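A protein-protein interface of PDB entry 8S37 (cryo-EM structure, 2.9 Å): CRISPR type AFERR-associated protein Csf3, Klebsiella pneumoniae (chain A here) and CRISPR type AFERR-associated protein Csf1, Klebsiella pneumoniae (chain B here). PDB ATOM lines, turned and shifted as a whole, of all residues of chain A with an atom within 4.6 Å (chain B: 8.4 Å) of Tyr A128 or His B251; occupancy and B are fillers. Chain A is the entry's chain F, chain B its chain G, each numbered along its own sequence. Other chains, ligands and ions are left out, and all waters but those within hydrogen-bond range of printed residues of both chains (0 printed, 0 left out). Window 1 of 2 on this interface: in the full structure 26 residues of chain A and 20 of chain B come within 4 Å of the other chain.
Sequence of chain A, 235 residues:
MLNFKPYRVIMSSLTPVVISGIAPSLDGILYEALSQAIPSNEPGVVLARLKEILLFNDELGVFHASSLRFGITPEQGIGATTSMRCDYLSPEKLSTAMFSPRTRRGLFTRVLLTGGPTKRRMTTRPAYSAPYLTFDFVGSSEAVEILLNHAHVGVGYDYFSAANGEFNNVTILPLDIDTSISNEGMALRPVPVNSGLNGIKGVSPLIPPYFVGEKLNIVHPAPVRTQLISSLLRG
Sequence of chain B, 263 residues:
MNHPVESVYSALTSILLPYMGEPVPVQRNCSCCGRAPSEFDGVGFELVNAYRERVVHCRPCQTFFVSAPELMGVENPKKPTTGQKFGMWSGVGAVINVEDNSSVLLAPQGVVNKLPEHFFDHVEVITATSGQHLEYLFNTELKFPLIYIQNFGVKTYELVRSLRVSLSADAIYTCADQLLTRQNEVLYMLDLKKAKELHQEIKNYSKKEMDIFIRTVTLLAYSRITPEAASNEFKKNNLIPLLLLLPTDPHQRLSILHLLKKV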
ATOM      1  N   PRO A  16      -5.428 -20.115  -9.537  1.00  0.00           N
ATOM      2  CA  PRO A  16      -6.338 -20.864 -10.410  1.00  0.00           C
ATOM      3  C   PRO A  16      -5.898 -20.799 -11.864  1.00  0.00           C
ATOM      4  O   PRO A  16      -5.409 -19.774 -12.340  1.00  0.00           O
ATOM      5  CB  PRO A  16      -7.681 -20.160 -10.202  1.00  0.00           C
ATOM      6  CG  PRO A  16      -7.582 -19.546  -8.869  1.00  0.00           C
ATOM      7  CD  PRO A  16      -6.157 -19.115  -8.737  1.00  0.00           C
ATOM      8  N   VAL A  17      -6.079 -21.913 -12.566  1.00  0.00           N
ATOM      9  CA  VAL A  17      -5.721 -22.032 -13.972  1.00  0.00           C
ATOM     10  C   VAL A  17      -6.956 -21.746 -14.809  1.00  0.00           C
ATOM     11  O   VAL A  17      -8.017 -22.341 -14.584  1.00  0.00           O
ATOM     12  CB  VAL A  17      -5.163 -23.428 -14.288  1.00  0.00           C
ATOM     13  CG1 VAL A  17      -4.884 -23.561 -15.774  1.00  0.00           C
ATOM     14  CG2 VAL A  17      -3.907 -23.694 -13.476  1.00  0.00           C
ATOM     15  N   ILE A  19      -8.491 -22.071 -18.476  1.00  0.00           N
ATOM     16  CA  ILE A  19      -8.296 -22.871 -19.678  1.00  0.00           C
ATOM     17  C   ILE A  19      -9.068 -22.215 -20.811  1.00  0.00           C
ATOM     18  O   ILE A  19     -10.279 -21.988 -20.699  1.00  0.00           O
ATOM     19  CB  ILE A  19      -8.752 -24.322 -19.465  1.00  0.00           C
ATOM     20  CG1 ILE A  19      -7.885 -24.990 -18.391  1.00  0.00           C
ATOM     21  CG2 ILE A  19      -8.705 -25.080 -20.789  1.00  0.00           C
ATOM     22  CD1 ILE A  19      -8.359 -26.363 -17.969  1.00  0.00           C
ATOM     23  N   PHE A  70      -4.635 -32.058 -14.556  1.00  0.00           N
ATOM     24  CA  PHE A  70      -4.517 -31.646 -13.165  1.00  0.00           C
ATOM     25  C   PHE A  70      -4.203 -32.848 -12.285  1.00  0.00           C
ATOM     26  O   PHE A  70      -4.895 -33.868 -12.335  1.00  0.00           O
ATOM     27  CB  PHE A  70      -5.811 -30.995 -12.687  1.00  0.00           C
ATOM     28  CG  PHE A  70      -6.146 -29.712 -13.383  1.00  0.00           C
ATOM     29  CD1 PHE A  70      -5.493 -28.541 -13.054  1.00  0.00           C
ATOM     30  CD2 PHE A  70      -7.134 -29.672 -14.347  1.00  0.00           C
ATOM     31  CE1 PHE A  70      -5.806 -27.358 -13.684  1.00  0.00           C
ATOM     32  CE2 PHE A  70      -7.453 -28.491 -14.979  1.00  0.00           C
ATOM     33  CZ  PHE A  70      -6.788 -27.333 -14.645  1.00  0.00           C
ATOM     34  N   ILE A  78      -9.701 -30.832  -7.791  1.00  0.00           N
ATOM     35  CA  ILE A  78     -10.040 -29.857  -8.816  1.00  0.00           C
ATOM     36  C   ILE A  78     -11.234 -29.043  -8.342  1.00  0.00           C
ATOM     37  O   ILE A  78     -12.261 -29.598  -7.932  1.00  0.00           O
ATOM     38  CB  ILE A  78     -10.318 -30.570 -10.150  1.00  0.00           C
ATOM     39  CG1 ILE A  78     -10.399 -29.570 -11.304  1.00  0.00           C
ATOM     40  CG2 ILE A  78     -11.600 -31.391 -10.080  1.00  0.00           C
ATOM     41  CD1 ILE A  78      -9.073 -28.979 -11.687  1.00  0.00           C
ATOM     42  N   GLY A  79     -11.092 -27.716  -8.367  1.00  0.00           N
ATOM     43  CA  GLY A  79     -12.131 -26.835  -7.885  1.00  0.00           C
ATOM     44  C   GLY A  79     -12.503 -25.796  -8.923  1.00  0.00           C
ATOM     45  O   GLY A  79     -11.727 -25.463  -9.815  1.00  0.00           O
ATOM     46  N   ALA A  80     -13.721 -25.283  -8.779  1.00  0.00           N
ATOM     47  CA  ALA A  80     -14.270 -24.254  -9.653  1.00  0.00           C
ATOM     48  C   ALA A  80     -14.123 -22.905  -8.960  1.00  0.00           C
ATOM     49  O   ALA A  80     -14.835 -22.618  -7.993  1.00  0.00           O
ATOM     50  CB  ALA A  80     -15.732 -24.541  -9.983  1.00  0.00           C
ATOM     51  N   THR A  81     -13.200 -22.086  -9.450  1.00  0.00           N
ATOM     52  CA  THR A  81     -12.948 -20.760  -8.913  1.00  0.00           C
ATOM     53  C   THR A  81     -13.036 -19.784 -10.072  1.00  0.00           C
ATOM     54  O   THR A  81     -12.979 -20.182 -11.232  1.00  0.00           O
ATOM     55  CB  THR A  81     -11.583 -20.665  -8.228  1.00  0.00           C
ATOM     56  OG1 THR A  81     -10.564 -21.113  -9.129  1.00  0.00           O
ATOM     57  CG2 THR A  81     -11.554 -21.520  -6.972  1.00  0.00           C
ATOM     58  N   PRO A 126     -13.999 -18.470 -15.841  1.00  0.00           N
ATOM     59  CA  PRO A 126     -13.802 -19.747 -15.151  1.00  0.00           C
ATOM     60  C   PRO A 126     -12.325 -20.062 -14.998  1.00  0.00           C
ATOM     61  O   PRO A 126     -11.532 -19.877 -15.922  1.00  0.00           O
ATOM     62  CB  PRO A 126     -14.501 -20.757 -16.065  1.00  0.00           C
ATOM     63  CG  PRO A 126     -15.507 -19.968 -16.776  1.00  0.00           C
ATOM     64  CD  PRO A 126     -14.903 -18.621 -16.990  1.00  0.00           C
ATOM     65  N   ALA A 127     -11.961 -20.537 -13.814  1.00  0.00           N
ATOM     66  CA  ALA A 127     -10.622 -20.993 -13.506  1.00  0.00           C
ATOM     67  C   ALA A 127     -10.729 -22.277 -12.701  1.00  0.00           C
ATOM     68  O   ALA A 127     -11.699 -22.489 -11.964  1.00  0.00           O
ATOM     69  CB  ALA A 127      -9.828 -19.943 -12.729  1.00  0.00           C
ATOM     70  N   TYR A 128      -9.713 -23.119 -12.837  1.00  0.00           N
ATOM     71  CA  TYR A 128      -9.657 -24.405 -12.165  1.00  0.00           C
ATOM     72  C   TYR A 128      -8.476 -24.400 -11.211  1.00  0.00           C
ATOM     73  O   TYR A 128      -7.349 -24.093 -11.614  1.00  0.00           O
ATOM     74  CB  TYR A 128      -9.533 -25.536 -13.178  1.00  0.00           C
ATOM     75  CG  TYR A 128     -10.553 -25.441 -14.279  1.00  0.00           C
ATOM     76  CD1 TYR A 128     -11.864 -25.825 -14.065  1.00  0.00           C
ATOM     77  CD2 TYR A 128     -10.207 -24.957 -15.529  1.00  0.00           C
ATOM     78  CE1 TYR A 128     -12.804 -25.735 -15.064  1.00  0.00           C
ATOM     79  CE2 TYR A 128     -11.141 -24.864 -16.538  1.00  0.00           C
ATOM     80  CZ  TYR A 128     -12.437 -25.257 -16.300  1.00  0.00           C
ATOM     81  OH  TYR A 128     -13.374 -25.168 -17.298  1.00  0.00           O
ATOM     82  N   SER A 129      -8.739 -24.736  -9.952  1.00  0.00           N
ATOM     83  CA  SER A 129      -7.766 -24.620  -8.871  1.00  0.00           C
ATOM     84  C   SER A 129      -7.492 -26.021  -8.342  1.00  0.00           C
ATOM     85  O   SER A 129      -8.157 -26.489  -7.414  1.00  0.00           O
ATOM     86  CB  SER A 129      -8.282 -23.701  -7.773  1.00  0.00           C
ATOM     87  OG  SER A 129      -9.494 -24.192  -7.231  1.00  0.00           O
ATOM     88  N   ALA A 130      -6.510 -26.682  -8.941  1.00  0.00           N
ATOM     89  CA  ALA A 130      -6.058 -27.993  -8.526  1.00  0.00           C
ATOM     90  C   ALA A 130      -4.726 -27.874  -7.794  1.00  0.00           C
ATOM     91  O   ALA A 130      -3.955 -26.948  -8.057  1.00  0.00           O
ATOM     92  CB  ALA A 130      -5.885 -28.929  -9.726  1.00  0.00           C
ATOM     93  N   VAL A 224     -10.441 -30.322 -18.963  1.00  0.00           N
ATOM     94  CA  VAL A 224     -10.151 -30.567 -17.556  1.00  0.00           C
ATOM     95  C   VAL A 224      -9.987 -32.067 -17.371  1.00  0.00           C
ATOM     96  O   VAL A 224     -10.972 -32.815 -17.381  1.00  0.00           O
ATOM     97  CB  VAL A 224     -11.247 -30.014 -16.637  1.00  0.00           C
ATOM     98  CG1 VAL A 224     -10.894 -30.283 -15.182  1.00  0.00           C
ATOM     99  CG2 VAL A 224     -11.432 -28.529 -16.879  1.00  0.00           C
ATOM    100  N   ARG B 182     -13.259 -18.024 -25.409  1.00  0.00           N
ATOM    101  CA  ARG B 182     -12.897 -19.428 -25.282  1.00  0.00           C
ATOM    102  C   ARG B 182     -12.547 -19.789 -23.846  1.00  0.00           C
ATOM    103  O   ARG B 182     -12.567 -20.974 -23.493  1.00  0.00           O
ATOM    104  CB  ARG B 182     -11.717 -19.751 -26.197  1.00  0.00           C
ATOM    105  CG  ARG B 182     -11.985 -19.537 -27.682  1.00  0.00           C
ATOM    106  CD  ARG B 182     -13.033 -20.496 -28.232  1.00  0.00           C
ATOM    107  NE  ARG B 182     -12.687 -21.894 -27.995  1.00  0.00           N
ATOM    108  CZ  ARG B 182     -11.796 -22.583 -28.697  1.00  0.00           C
ATOM    109  NH1 ARG B 182     -11.115 -22.031 -29.690  1.00  0.00           N
ATOM    110  NH2 ARG B 182     -11.579 -23.859 -28.394  1.00  0.00           N
ATOM    111  N   GLN B 183     -12.231 -18.798 -23.011  1.00  0.00           N
ATOM    112  CA  GLN B 183     -11.903 -19.052 -21.617  1.00  0.00           C
ATOM    113  C   GLN B 183     -13.131 -19.180 -20.731  1.00  0.00           C
ATOM    114  O   GLN B 183     -13.007 -19.669 -19.603  1.00  0.00           O
ATOM    115  CB  GLN B 183     -11.014 -17.931 -21.078  1.00  0.00           C
ATOM    116  CG  GLN B 183      -9.831 -17.601 -21.963  1.00  0.00           C
ATOM    117  CD  GLN B 183     -10.127 -16.490 -22.946  1.00  0.00           C
ATOM    118  OE1 GLN B 183     -10.394 -15.355 -22.554  1.00  0.00           O
ATOM    119  NE2 GLN B 183     -10.089 -16.813 -24.233  1.00  0.00           N
ATOM    120  N   ASN B 184     -14.307 -18.756 -21.207  1.00  0.00           N
ATOM    121  CA  ASN B 184     -15.518 -18.791 -20.395  1.00  0.00           C
ATOM    122  C   ASN B 184     -16.692 -19.424 -21.128  1.00  0.00           C
ATOM    123  O   ASN B 184     -17.841 -19.218 -20.728  1.00  0.00           O
ATOM    124  CB  ASN B 184     -15.897 -17.384 -19.929  1.00  0.00           C
ATOM    125  CG  ASN B 184     -16.342 -16.497 -21.068  1.00  0.00           C
ATOM    126  OD1 ASN B 184     -15.907 -16.667 -22.206  1.00  0.00           O
ATOM    127  ND2 ASN B 184     -17.210 -15.540 -20.769  1.00  0.00           N
ATOM    128  N   GLU B 185     -16.438 -20.191 -22.184  1.00  0.00           N
ATOM    129  CA  GLU B 185     -17.525 -20.936 -22.798  1.00  0.00           C
ATOM    130  C   GLU B 185     -17.904 -22.173 -22.001  1.00  0.00           C
ATOM    131  O   GLU B 185     -18.973 -22.740 -22.247  1.00  0.00           O
ATOM    132  CB  GLU B 185     -17.143 -21.341 -24.224  1.00  0.00           C
ATOM    133  CG  GLU B 185     -15.952 -22.286 -24.314  1.00  0.00           C
ATOM    134  CD  GLU B 185     -15.527 -22.548 -25.745  1.00  0.00           C
ATOM    135  OE1 GLU B 185     -16.140 -21.968 -26.665  1.00  0.00           O
ATOM    136  OE2 GLU B 185     -14.579 -23.336 -25.949  1.00  0.00           O
ATOM    137  N   VAL B 186     -17.075 -22.593 -21.043  1.00  0.00           N
ATOM    138  CA  VAL B 186     -17.455 -23.710 -20.186  1.00  0.00           C
ATOM    139  C   VAL B 186     -18.622 -23.323 -19.289  1.00  0.00           C
ATOM    140  O   VAL B 186     -19.497 -24.146 -18.996  1.00  0.00           O
ATOM    141  CB  VAL B 186     -16.246 -24.196 -19.365  1.00  0.00           C
ATOM    142  CG1 VAL B 186     -15.780 -23.124 -18.390  1.00  0.00           C
ATOM    143  CG2 VAL B 186     -16.594 -25.479 -18.630  1.00  0.00           C
ATOM    144  N   LEU B 187     -18.662 -22.067 -18.841  1.00  0.00           N
ATOM    145  CA  LEU B 187     -19.786 -21.605 -18.036  1.00  0.00           C
ATOM    146  C   LEU B 187     -21.047 -21.414 -18.859  1.00  0.00           C
ATOM    147  O   LEU B 187     -22.131 -21.301 -18.279  1.00  0.00           O
ATOM    148  CB  LEU B 187     -19.447 -20.288 -17.333  1.00  0.00           C
ATOM    149  CG  LEU B 187     -19.079 -20.345 -15.848  1.00  0.00           C
ATOM    150  CD1 LEU B 187     -18.744 -18.950 -15.346  1.00  0.00           C
ATOM    151  CD2 LEU B 187     -20.198 -20.946 -15.008  1.00  0.00           C
ATOM    152  N   TYR B 188     -20.930 -21.375 -20.187  1.00  0.00           N
ATOM    153  CA  TYR B 188     -22.067 -21.199 -21.079  1.00  0.00           C
ATOM    154  C   TYR B 188     -22.270 -22.408 -21.981  1.00  0.00           C
ATOM    155  O   TYR B 188     -22.942 -22.301 -23.011  1.00  0.00           O
ATOM    156  CB  TYR B 188     -21.879 -19.930 -21.910  1.00  0.00           C
ATOM    157  CG  TYR B 188     -21.643 -18.699 -21.066  1.00  0.00           C
ATOM    158  CD1 TYR B 188     -22.381 -18.474 -19.912  1.00  0.00           C
ATOM    159  CD2 TYR B 188     -20.672 -17.772 -21.409  1.00  0.00           C
ATOM    160  CE1 TYR B 188     -22.168 -17.360 -19.134  1.00  0.00           C
ATOM    161  CE2 TYR B 188     -20.451 -16.653 -20.636  1.00  0.00           C
ATOM    162  CZ  TYR B 188     -21.202 -16.452 -19.499  1.00  0.00           C
ATOM    163  OH  TYR B 188     -20.989 -15.341 -18.719  1.00  0.00           O
ATOM    164  N   MET B 189     -21.705 -23.555 -21.613  1.00  0.00           N
ATOM    165  CA  MET B 189     -21.911 -24.808 -22.322  1.00  0.00           C
ATOM    166  C   MET B 189     -22.770 -25.706 -21.447  1.00  0.00           C
ATOM    167  O   MET B 189     -22.405 -25.998 -20.304  1.00  0.00           O
ATOM    168  CB  MET B 189     -20.576 -25.482 -22.642  1.00  0.00           C
ATOM    169  CG  MET B 189     -20.656 -26.619 -23.644  1.00  0.00           C
ATOM    170  SD  MET B 189     -20.400 -26.078 -25.347  1.00  0.00           S
ATOM    171  CE  MET B 189     -21.992 -25.359 -25.738  1.00  0.00           C
ATOM    172  N   LEU B 190     -23.905 -26.137 -21.987  1.00  0.00           N
ATOM    173  CA  LEU B 190     -24.831 -27.027 -21.300  1.00  0.00           C
ATOM    174  C   LEU B 190     -24.833 -28.358 -22.035  1.00  0.00           C
ATOM    175  O   LEU B 190     -25.171 -28.414 -23.222  1.00  0.00           O
ATOM    176  CB  LEU B 190     -26.235 -26.424 -21.252  1.00  0.00           C
ATOM    177  CG  LEU B 190     -27.169 -26.855 -20.116  1.00  0.00           C
ATOM    178  CD1 LEU B 190     -27.415 -28.357 -20.134  1.00  0.00           C
ATOM    179  CD2 LEU B 190     -26.623 -26.416 -18.763  1.00  0.00           C
ATOM    180  N   ALA B 221     -16.608 -29.461  -5.921  1.00  0.00           N
ATOM    181  CA  ALA B 221     -16.360 -28.536  -7.019  1.00  0.00           C
ATOM    182  C   ALA B 221     -15.946 -27.165  -6.509  1.00  0.00           C
ATOM    183  O   ALA B 221     -15.216 -26.446  -7.196  1.00  0.00           O
ATOM    184  CB  ALA B 221     -17.605 -28.420  -7.896  1.00  0.00           C
ATOM    185  N   TYR B 222     -16.397 -26.783  -5.317  1.00  0.00           N
ATOM    186  CA  TYR B 222     -15.931 -25.566  -4.669  1.00  0.00           C
ATOM    187  C   TYR B 222     -14.754 -25.821  -3.737  1.00  0.00           C
ATOM    188  O   TYR B 222     -14.330 -24.906  -3.027  1.00  0.00           O
ATOM    189  CB  TYR B 222     -17.071 -24.911  -3.889  1.00  0.00           C
ATOM    190  CG  TYR B 222     -18.106 -24.244  -4.763  1.00  0.00           C
ATOM    191  CD1 TYR B 222     -17.809 -23.082  -5.457  1.00  0.00           C
ATOM    192  CD2 TYR B 222     -19.383 -24.768  -4.881  1.00  0.00           C
ATOM    193  CE1 TYR B 222     -18.750 -22.466  -6.254  1.00  0.00           C
ATOM    194  CE2 TYR B 222     -20.333 -24.159  -5.675  1.00  0.00           C
ATOM    195  CZ  TYR B 222     -20.011 -23.008  -6.359  1.00  0.00           C
ATOM    196  OH  TYR B 222     -20.955 -22.398  -7.151  1.00  0.00           O
ATOM    197  N   PRO B 247     -19.001 -34.852 -15.966  1.00  0.00           N
ATOM    198  CA  PRO B 247     -17.729 -34.412 -16.546  1.00  0.00           C
ATOM    199  C   PRO B 247     -16.710 -34.110 -15.461  1.00  0.00           C
ATOM    200  O   PRO B 247     -17.046 -33.631 -14.376  1.00  0.00           O
ATOM    201  CB  PRO B 247     -18.104 -33.146 -17.323  1.00  0.00           C
ATOM    202  CG  PRO B 247     -19.549 -33.254 -17.563  1.00  0.00           C
ATOM    203  CD  PRO B 247     -20.108 -33.974 -16.382  1.00  0.00           C
ATOM    204  N   THR B 248     -15.446 -34.408 -15.764  1.00  0.00           N
ATOM    205  CA  THR B 248     -14.375 -34.122 -14.818  1.00  0.00           C
ATOM    206  C   THR B 248     -14.277 -32.632 -14.518  1.00  0.00           C
ATOM    207  O   THR B 248     -13.843 -32.248 -13.426  1.00  0.00           O
ATOM    208  CB  THR B 248     -13.046 -34.638 -15.365  1.00  0.00           C
ATOM    209  OG1 THR B 248     -13.164 -36.034 -15.669  1.00  0.00           O
ATOM    210  CG2 THR B 248     -11.935 -34.440 -14.350  1.00  0.00           C
ATOM    211  N   ASP B 249     -14.660 -31.788 -15.467  1.00  0.00           N
ATOM    212  CA  ASP B 249     -14.588 -30.349 -15.268  1.00  0.00           C
ATOM    213  C   ASP B 249     -15.477 -29.944 -14.092  1.00  0.00           C
ATOM    214  O   ASP B 249     -16.665 -30.291 -14.078  1.00  0.00           O
ATOM    215  CB  ASP B 249     -15.021 -29.625 -16.543  1.00  0.00           C
ATOM    216  CG  ASP B 249     -14.858 -28.117 -16.455  1.00  0.00           C
ATOM    217  OD1 ASP B 249     -15.390 -27.495 -15.511  1.00  0.00           O
ATOM    218  OD2 ASP B 249     -14.195 -27.547 -17.346  1.00  0.00           O
ATOM    219  N   PRO B 250     -14.957 -29.214 -13.098  1.00  0.00           N
ATOM    220  CA  PRO B 250     -15.819 -28.834 -11.971  1.00  0.00           C
ATOM    221  C   PRO B 250     -16.893 -27.831 -12.347  1.00  0.00           C
ATOM    222  O   PRO B 250     -17.982 -27.868 -11.765  1.00  0.00           O
ATOM    223  CB  PRO B 250     -14.827 -28.250 -10.959  1.00  0.00           C
ATOM    224  CG  PRO B 250     -13.748 -27.703 -11.794  1.00  0.00           C
ATOM    225  CD  PRO B 250     -13.597 -28.675 -12.929  1.00  0.00           C
ATOM    226  N   HIS B 251     -16.627 -26.927 -13.290  1.00  0.00           N
ATOM    227  CA  HIS B 251     -17.662 -25.984 -13.699  1.00  0.00           C
ATOM    228  C   HIS B 251     -18.781 -26.695 -14.446  1.00  0.00           C
ATOM    229  O   HIS B 251     -19.957 -26.349 -14.289  1.00  0.00           O
ATOM    230  CB  HIS B 251     -17.060 -24.867 -14.547  1.00  0.00           C
ATOM    231  CG  HIS B 251     -16.498 -23.743 -13.738  1.00  0.00           C
ATOM    232  ND1 HIS B 251     -15.146 -23.582 -13.522  1.00  0.00           N
ATOM    233  CD2 HIS B 251     -17.107 -22.732 -13.076  1.00  0.00           C
ATOM    234  CE1 HIS B 251     -14.946 -22.515 -12.772  1.00  0.00           C
ATOM    235  NE2 HIS B 251     -16.120 -21.981 -12.486  1.00  0.00           N
ATOM    236  N   GLN B 252     -18.439 -27.698 -15.253  1.00  0.00           N
ATOM    237  CA  GLN B 252     -19.473 -28.522 -15.869  1.00  0.00           C
ATOM    238  C   GLN B 252     -20.278 -29.252 -14.805  1.00  0.00           C
ATOM    239  O   GLN B 252     -21.503 -29.375 -14.917  1.00  0.00           O
ATOM    240  CB  GLN B 252     -18.848 -29.519 -16.841  1.00  0.00           C
ATOM    241  CG  GLN B 252     -18.186 -28.887 -18.052  1.00  0.00           C
ATOM    242  CD  GLN B 252     -19.186 -28.435 -19.094  1.00  0.00           C
ATOM    243  OE1 GLN B 252     -20.112 -27.682 -18.799  1.00  0.00           O
ATOM    244  NE2 GLN B 252     -19.005 -28.898 -20.325  1.00  0.00           N
ATOM    245  N   ARG B 253     -19.603 -29.755 -13.771  1.00  0.00           N
ATOM    246  CA  ARG B 253     -20.305 -30.393 -12.663  1.00  0.00           C
ATOM    247  C   ARG B 253     -21.287 -29.428 -12.015  1.00  0.00           C
ATOM    248  O   ARG B 253     -22.438 -29.785 -11.747  1.00  0.00           O
ATOM    249  CB  ARG B 253     -19.306 -30.908 -11.631  1.00  0.00           C
ATOM    250  CG  ARG B 253     -18.581 -32.167 -12.044  1.00  0.00           C
ATOM    251  CD  ARG B 253     -17.651 -32.637 -10.947  1.00  0.00           C
ATOM    252  NE  ARG B 253     -17.118 -33.967 -11.211  1.00  0.00           N
ATOM    253  CZ  ARG B 253     -16.295 -34.622 -10.404  1.00  0.00           C
ATOM    254  NH1 ARG B 253     -15.874 -34.094  -9.266  1.00  0.00           N
ATOM    255  NH2 ARG B 253     -15.884 -35.839 -10.747  1.00  0.00           N
ATOM    256  N   LEU B 254     -20.846 -28.199 -11.744  1.00  0.00           N
ATOM    257  CA  LEU B 254     -21.725 -27.227 -11.102  1.00  0.00           C
ATOM    258  C   LEU B 254     -22.903 -26.877 -11.999  1.00  0.00           C
ATOM    259  O   LEU B 254     -24.038 -26.749 -11.525  1.00  0.00           O
ATOM    260  CB  LEU B 254     -20.939 -25.968 -10.740  1.00  0.00           C
ATOM    261  CG  LEU B 254     -19.895 -26.106  -9.632  1.00  0.00           C
ATOM    262  CD1 LEU B 254     -19.103 -24.819  -9.507  1.00  0.00           C
ATOM    263  CD2 LEU B 254     -20.547 -26.462  -8.307  1.00  0.00           C
ATOM    264  N   SER B 255     -22.657 -26.722 -13.300  1.00  0.00           N
ATOM    265  CA  SER B 255     -23.746 -26.429 -14.225  1.00  0.00           C
ATOM    266  C   SER B 255     -24.756 -27.569 -14.254  1.00  0.00           C
ATOM    267  O   SER B 255     -25.969 -27.337 -14.213  1.00  0.00           O
ATOM    268  CB  SER B 255     -23.189 -26.169 -15.623  1.00  0.00           C
ATOM    269  OG  SER B 255     -22.345 -25.032 -15.628  1.00  0.00           O
ATOM    270  N   ILE B 256     -24.274 -28.809 -14.313  1.00  0.00           N
ATOM    271  CA  ILE B 256     -25.184 -29.943 -14.399  1.00  0.00           C
ATOM    272  C   ILE B 256     -25.921 -30.138 -13.081  1.00  0.00           C
ATOM    273  O   ILE B 256     -27.077 -30.574 -13.068  1.00  0.00           O
ATOM    274  CB  ILE B 256     -24.406 -31.206 -14.810  1.00  0.00           C
ATOM    275  CG1 ILE B 256     -23.905 -31.073 -16.251  1.00  0.00           C
ATOM    276  CG2 ILE B 256     -25.280 -32.438 -14.663  1.00  0.00           C
ATOM    277  CD1 ILE B 256     -22.749 -31.987 -16.585  1.00  0.00           C
ATOM    278  N   LEU B 257     -25.290 -29.798 -11.958  1.00  0.00           N
ATOM    279  CA  LEU B 257     -25.992 -29.835 -10.681  1.00  0.00           C
ATOM    280  C   LEU B 257     -27.087 -28.782 -10.631  1.00  0.00           C
ATOM    281  O   LEU B 257     -28.191 -29.050 -10.143  1.00  0.00           O
ATOM    282  CB  LEU B 257     -25.010 -29.631  -9.532  1.00  0.00           C
ATOM    283  CG  LEU B 257     -24.064 -30.786  -9.210  1.00  0.00           C
ATOM    284  CD1 LEU B 257     -23.024 -30.298  -8.222  1.00  0.00           C
ATOM    285  CD2 LEU B 257     -24.816 -31.989  -8.660  1.00  0.00           C
ATOM    286  N   HIS B 258     -26.779 -27.563 -11.079  1.00  0.00           N
ATOM    287  CA  HIS B 258     -27.801 -26.531 -11.206  1.00  0.00           C
ATOM    288  C   HIS B 258     -28.955 -27.023 -12.065  1.00  0.00           C
ATOM    289  O   HIS B 258     -30.129 -26.805 -11.739  1.00  0.00           O
ATOM    290  CB  HIS B 258     -27.183 -25.267 -11.801  1.00  0.00           C
ATOM    291  CG  HIS B 258     -28.123 -24.106 -11.870  1.00  0.00           C
ATOM    292  ND1 HIS B 258     -28.125 -23.213 -12.920  1.00  0.00           N
ATOM    293  CD2 HIS B 258     -29.084 -23.683 -11.016  1.00  0.00           C
ATOM    294  CE1 HIS B 258     -29.052 -22.296 -12.714  1.00  0.00           C
ATOM    295  NE2 HIS B 258     -29.647 -22.556 -11.564  1.00  0.00           N
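OD2 of Asp B249 is in hydrogen-bond range of OH of Tyr A128. N of Ala A80 lies within hydrogen-bond range of O of Ala B221 (2.5 Å).
The side-chain hydroxyl of Ser B255 is in hydrogen-bond range of the backbone carbonyl oxygen of His B251. The guanidinium group (NE) of Arg B182 is in salt-bridge range of the side-chain carboxylate (OE2) of Glu B185, at 3.1 Å. N of His B251 is in hydrogen-bond range of OD1 of Asp B249 (2.6 Å). The backbone carbonyl oxygen (O) of Gly A79 lies within hydrogen-bond range of the backbone NH (N) of Ser A129, at 3.1 Å. N of Ala A127 sits at hydrogen-bond distance from O of Thr A81, 2.8 Å away. O of Val A17 is in hydrogen-bond range of N of Tyr A128, 2.6 Å away.
Arg B182 touches Ile A19 (O to O, 3.8 Å). Pro B250 touches Ile A78. Ala B221 touches Gly A79 (O to CA, 3.2 Å). Ala A80 touches Leu B254. CE1 of His B251 touches O of Thr A81, at 3.4 Å. Ala A127 touches His B251. OH of Tyr A128 touches CG1 of Val B186, at 3.3 Å. Pro B250 touches Tyr A128. His B251 touches Tyr A128. Val A224 touches Thr B248.
His B251 touches just these residues of chain A: Ala A80, Thr A81, Pro A126, Ala A127 and Tyr A128. Ala A127 touches just one residue of chain B: His B251. No residue of chain B comes within 4 Å of Ser A129. Printed residues of chain A within 4 Å of Leu B254: Ala A80. Printed residues of chain B within 4 Å of Ile A78: Pro B250. Printed residues of chain B within 4 Å of Thr A81: His B251 (3.4 Å). Of the printed residues of chain B, Gly A79 touches Ala B221 (3.2 Å) and Pro B250 (3.6 Å). His B258 touches none of the printed residues of chain A. The nearest printed residue of chain B that does not touch Tyr A128 is Gln B252 (6.0 Å). The nearest printed residue of chain A that does not touch His B251 is Gly A79 (5.3 Å).
Of the 23 printed residues of chain B, 12 touch a printed residue of chain A. Among the printed residues, 24 pairs touch across the chains.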
